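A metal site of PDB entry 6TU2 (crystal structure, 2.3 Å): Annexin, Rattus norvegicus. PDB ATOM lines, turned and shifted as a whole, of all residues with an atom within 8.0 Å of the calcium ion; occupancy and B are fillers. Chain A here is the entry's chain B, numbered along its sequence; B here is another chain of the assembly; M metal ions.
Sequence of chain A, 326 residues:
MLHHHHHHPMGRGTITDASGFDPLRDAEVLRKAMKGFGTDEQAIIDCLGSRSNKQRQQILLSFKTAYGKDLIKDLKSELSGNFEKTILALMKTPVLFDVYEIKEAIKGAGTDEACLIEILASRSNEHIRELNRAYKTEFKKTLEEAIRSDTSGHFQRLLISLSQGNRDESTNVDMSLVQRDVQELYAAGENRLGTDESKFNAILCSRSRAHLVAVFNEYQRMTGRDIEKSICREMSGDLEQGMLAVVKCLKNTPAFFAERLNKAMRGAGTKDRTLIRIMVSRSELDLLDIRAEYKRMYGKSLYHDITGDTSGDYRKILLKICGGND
Leu 193 touches the calcium ion. Within 4 Å of the calcium ion: Gly 189, Arg 192, Leu 193, Gly 194 and Glu 234. Along chain A the residues within 4 Å of the calcium ion span positions 189 to 234. The nearest printed residue that does not touch the calcium ion is Thr 195 (4.5 Å).
O of Glu 234 lies within hydrogen-bond range of OG1 of Thr 195 (3.2 Å).
The calcium ion is bound by the backbone carbonyl oxygen (O) of Gly 194, the backbone carbonyl oxygen (O) of Arg 192, the backbone carbonyl oxygen (O) of Gly 189 and the side-chain carboxylate (OE2) of Glu 234. The calcium ion has four donor atoms within binding distance. Slightly farther from the calcium ion lies the side-chain carboxylate (OE1) of Glu 234 (3.0 Å).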
ATOM      1  N   TYR A 186      17.142  23.644   7.310  1.00  0.00           N
ATOM      2  CA  TYR A 186      16.781  23.508   5.895  1.00  0.00           C
ATOM      3  C   TYR A 186      15.663  22.493   5.704  1.00  0.00           C
ATOM      4  O   TYR A 186      14.744  22.710   4.920  1.00  0.00           O
ATOM      5  CB  TYR A 186      18.024  23.115   5.088  1.00  0.00           C
ATOM      6  CG  TYR A 186      17.850  23.183   3.586  1.00  0.00           C
ATOM      7  CD1 TYR A 186      17.262  24.288   2.989  1.00  0.00           C
ATOM      8  CD2 TYR A 186      18.293  22.157   2.764  1.00  0.00           C
ATOM      9  CE1 TYR A 186      17.107  24.362   1.613  1.00  0.00           C
ATOM     10  CE2 TYR A 186      18.148  22.222   1.394  1.00  0.00           C
ATOM     11  CZ  TYR A 186      17.554  23.324   0.819  1.00  0.00           C
ATOM     12  OH  TYR A 186      17.405  23.402  -0.546  1.00  0.00           O
ATOM     13  N   ALA A 187      15.723  21.388   6.452  1.00  0.00           N
ATOM     14  CA  ALA A 187      14.688  20.354   6.350  1.00  0.00           C
ATOM     15  C   ALA A 187      13.364  20.802   6.967  1.00  0.00           C
ATOM     16  O   ALA A 187      12.318  20.280   6.579  1.00  0.00           O
ATOM     17  CB  ALA A 187      15.164  19.071   7.014  1.00  0.00           C
ATOM     18  N   ALA A 188      13.410  21.738   7.905  1.00  0.00           N
ATOM     19  CA  ALA A 188      12.196  22.223   8.564  1.00  0.00           C
ATOM     20  C   ALA A 188      11.468  23.291   7.760  1.00  0.00           C
ATOM     21  O   ALA A 188      10.313  23.592   8.073  1.00  0.00           O
ATOM     22  CB  ALA A 188      12.540  22.776   9.949  1.00  0.00           C
ATOM     23  N   GLY A 189      12.104  23.847   6.732  1.00  0.00           N
ATOM     24  CA  GLY A 189      11.506  24.936   5.982  1.00  0.00           C
ATOM     25  C   GLY A 189      11.574  24.792   4.479  1.00  0.00           C
ATOM     26  O   GLY A 189      10.691  24.193   3.858  1.00  0.00           O
ATOM     27  N   GLU A 190      12.640  25.332   3.877  1.00  0.00           N
ATOM     28  CA  GLU A 190      12.688  25.434   2.430  1.00  0.00           C
ATOM     29  C   GLU A 190      12.796  24.075   1.754  1.00  0.00           C
ATOM     30  O   GLU A 190      12.308  23.911   0.633  1.00  0.00           O
ATOM     31  CB  GLU A 190      13.856  26.330   2.001  1.00  0.00           C
ATOM     32  CG  GLU A 190      13.600  27.805   2.199  1.00  0.00           C
ATOM     33  CD  GLU A 190      14.473  28.678   1.323  1.00  0.00           C
ATOM     34  OE1 GLU A 190      15.596  29.009   1.741  1.00  0.00           O
ATOM     35  OE2 GLU A 190      14.034  29.018   0.205  1.00  0.00           O
ATOM     36  N   ASN A 191      13.438  23.099   2.407  1.00  0.00           N
ATOM     37  CA  ASN A 191      13.602  21.776   1.824  1.00  0.00           C
ATOM     38  C   ASN A 191      12.494  20.810   2.208  1.00  0.00           C
ATOM     39  O   ASN A 191      12.747  19.610   2.339  1.00  0.00           O
ATOM     40  CB  ASN A 191      14.964  21.193   2.226  1.00  0.00           C
ATOM     41  CG  ASN A 191      15.436  20.109   1.279  1.00  0.00           C
ATOM     42  OD1 ASN A 191      15.020  20.057   0.116  1.00  0.00           O
ATOM     43  ND2 ASN A 191      16.299  19.222   1.766  1.00  0.00           N
ATOM     44  N   ARG A 192      11.275  21.292   2.410  1.00  0.00           N
ATOM     45  CA  ARG A 192      10.166  20.399   2.732  1.00  0.00           C
ATOM     46  C   ARG A 192       8.858  21.066   2.326  1.00  0.00           C
ATOM     47  O   ARG A 192       8.833  22.216   1.861  1.00  0.00           O
ATOM     48  CB  ARG A 192      10.169  20.034   4.217  1.00  0.00           C
ATOM     49  CG  ARG A 192       9.512  21.045   5.146  1.00  0.00           C
ATOM     50  CD  ARG A 192       9.371  20.477   6.552  1.00  0.00           C
ATOM     51  NE  ARG A 192       7.979  20.201   6.899  1.00  0.00           N
ATOM     52  CZ  ARG A 192       7.596  19.482   7.944  1.00  0.00           C
ATOM     53  NH1 ARG A 192       8.501  18.944   8.757  1.00  0.00           N
ATOM     54  NH2 ARG A 192       6.304  19.295   8.188  1.00  0.00           N
ATOM     55  N   LEU A 193       7.775  20.337   2.517  1.00  0.00           N
ATOM     56  CA  LEU A 193       6.427  20.813   2.226  1.00  0.00           C
ATOM     57  C   LEU A 193       5.744  21.155   3.534  1.00  0.00           C
ATOM     58  O   LEU A 193       5.696  20.328   4.455  1.00  0.00           O
ATOM     59  CB  LEU A 193       5.644  19.751   1.455  1.00  0.00           C
ATOM     60  CG  LEU A 193       6.303  19.455   0.101  1.00  0.00           C
ATOM     61  CD1 LEU A 193       5.814  18.152  -0.500  1.00  0.00           C
ATOM     62  CD2 LEU A 193       6.036  20.627  -0.835  1.00  0.00           C
ATOM     63  N   GLY A 194       5.222  22.373   3.626  1.00  0.00           N
ATOM     64  CA  GLY A 194       4.789  22.896   4.897  1.00  0.00           C
ATOM     65  C   GLY A 194       5.980  23.421   5.683  1.00  0.00           C
ATOM     66  O   GLY A 194       7.050  23.695   5.139  1.00  0.00           O
ATOM     67  N   THR A 195       5.776  23.546   6.997  1.00  0.00           N
ATOM     68  CA  THR A 195       6.822  24.077   7.860  1.00  0.00           C
ATOM     69  C   THR A 195       6.763  23.380   9.206  1.00  0.00           C
ATOM     70  O   THR A 195       5.680  23.137   9.746  1.00  0.00           O
ATOM     71  CB  THR A 195       6.668  25.602   8.047  1.00  0.00           C
ATOM     72  OG1 THR A 195       6.552  26.235   6.761  1.00  0.00           O
ATOM     73  CG2 THR A 195       7.867  26.173   8.786  1.00  0.00           C
ATOM     74  N   ASP A 196       7.936  23.060   9.740  1.00  0.00           N
ATOM     75  CA  ASP A 196       8.073  22.581  11.119  1.00  0.00           C
ATOM     76  C   ASP A 196       8.509  23.775  11.968  1.00  0.00           C
ATOM     77  O   ASP A 196       9.676  23.925  12.333  1.00  0.00           O
ATOM     78  CB  ASP A 196       9.053  21.422  11.200  1.00  0.00           C
ATOM     79  CG  ASP A 196       9.226  20.895  12.620  1.00  0.00           C
ATOM     80  OD1 ASP A 196       8.507  21.374  13.531  1.00  0.00           O
ATOM     81  OD2 ASP A 196      10.087  20.012  12.838  1.00  0.00           O
ATOM     82  N   SER A 230      14.856  32.406   4.243  1.00  0.00           N
ATOM     83  CA  SER A 230      14.071  31.185   4.455  1.00  0.00           C
ATOM     84  C   SER A 230      12.919  31.431   5.412  1.00  0.00           C
ATOM     85  O   SER A 230      11.821  30.890   5.226  1.00  0.00           O
ATOM     86  CB  SER A 230      14.969  30.068   4.984  1.00  0.00           C
ATOM     87  OG  SER A 230      16.012  29.762   4.073  1.00  0.00           O
ATOM     88  N   ARG A 233       9.752  33.164   3.802  1.00  0.00           N
ATOM     89  CA  ARG A 233       8.921  32.374   2.903  1.00  0.00           C
ATOM     90  C   ARG A 233       8.191  31.249   3.618  1.00  0.00           C
ATOM     91  O   ARG A 233       7.120  30.839   3.158  1.00  0.00           O
ATOM     92  CB  ARG A 233       9.769  31.803   1.777  1.00  0.00           C
ATOM     93  CG  ARG A 233      10.345  32.879   0.878  1.00  0.00           C
ATOM     94  CD  ARG A 233      11.397  32.360  -0.061  1.00  0.00           C
ATOM     95  NE  ARG A 233      12.115  33.467  -0.684  1.00  0.00           N
ATOM     96  CZ  ARG A 233      13.195  33.335  -1.450  1.00  0.00           C
ATOM     97  NH1 ARG A 233      13.687  32.136  -1.714  1.00  0.00           N
ATOM     98  NH2 ARG A 233      13.765  34.414  -1.974  1.00  0.00           N
ATOM     99  N   GLU A 234       8.736  30.752   4.717  1.00  0.00           N
ATOM    100  CA  GLU A 234       8.084  29.684   5.467  1.00  0.00           C
ATOM    101  C   GLU A 234       7.125  30.206   6.523  1.00  0.00           C
ATOM    102  O   GLU A 234       6.273  29.437   6.999  1.00  0.00           O
ATOM    103  CB  GLU A 234       9.136  28.806   6.142  1.00  0.00           C
ATOM    104  CG  GLU A 234      10.011  28.022   5.160  1.00  0.00           C
ATOM    105  CD  GLU A 234       9.199  27.083   4.289  1.00  0.00           C
ATOM    106  OE1 GLU A 234       9.560  26.905   3.110  1.00  0.00           O
ATOM    107  OE2 GLU A 234       8.195  26.524   4.784  1.00  0.00           O
ATOM    108  N   LYS B  32      -0.205  33.145  -5.182  1.00  0.00           N
ATOM    109  CA  LYS B  32      -0.788  32.866  -3.876  1.00  0.00           C
ATOM    110  C   LYS B  32      -1.595  34.061  -3.361  1.00  0.00           C
ATOM    111  O   LYS B  32      -2.567  33.880  -2.633  1.00  0.00           O
ATOM    112  CB  LYS B  32       0.301  32.496  -2.881  1.00  0.00           C
ATOM    113  CG  LYS B  32       0.797  31.057  -3.019  1.00  0.00           C
ATOM    114  CD  LYS B  32       2.119  30.831  -2.298  1.00  0.00           C
ATOM    115  CE  LYS B  32       2.591  29.391  -2.465  1.00  0.00           C
ATOM    116  NZ  LYS B  32       3.923  29.168  -1.820  1.00  0.00           N
HETATM  117 CA    CA M   1       8.017  24.328   3.015  1.00  0.00          CA
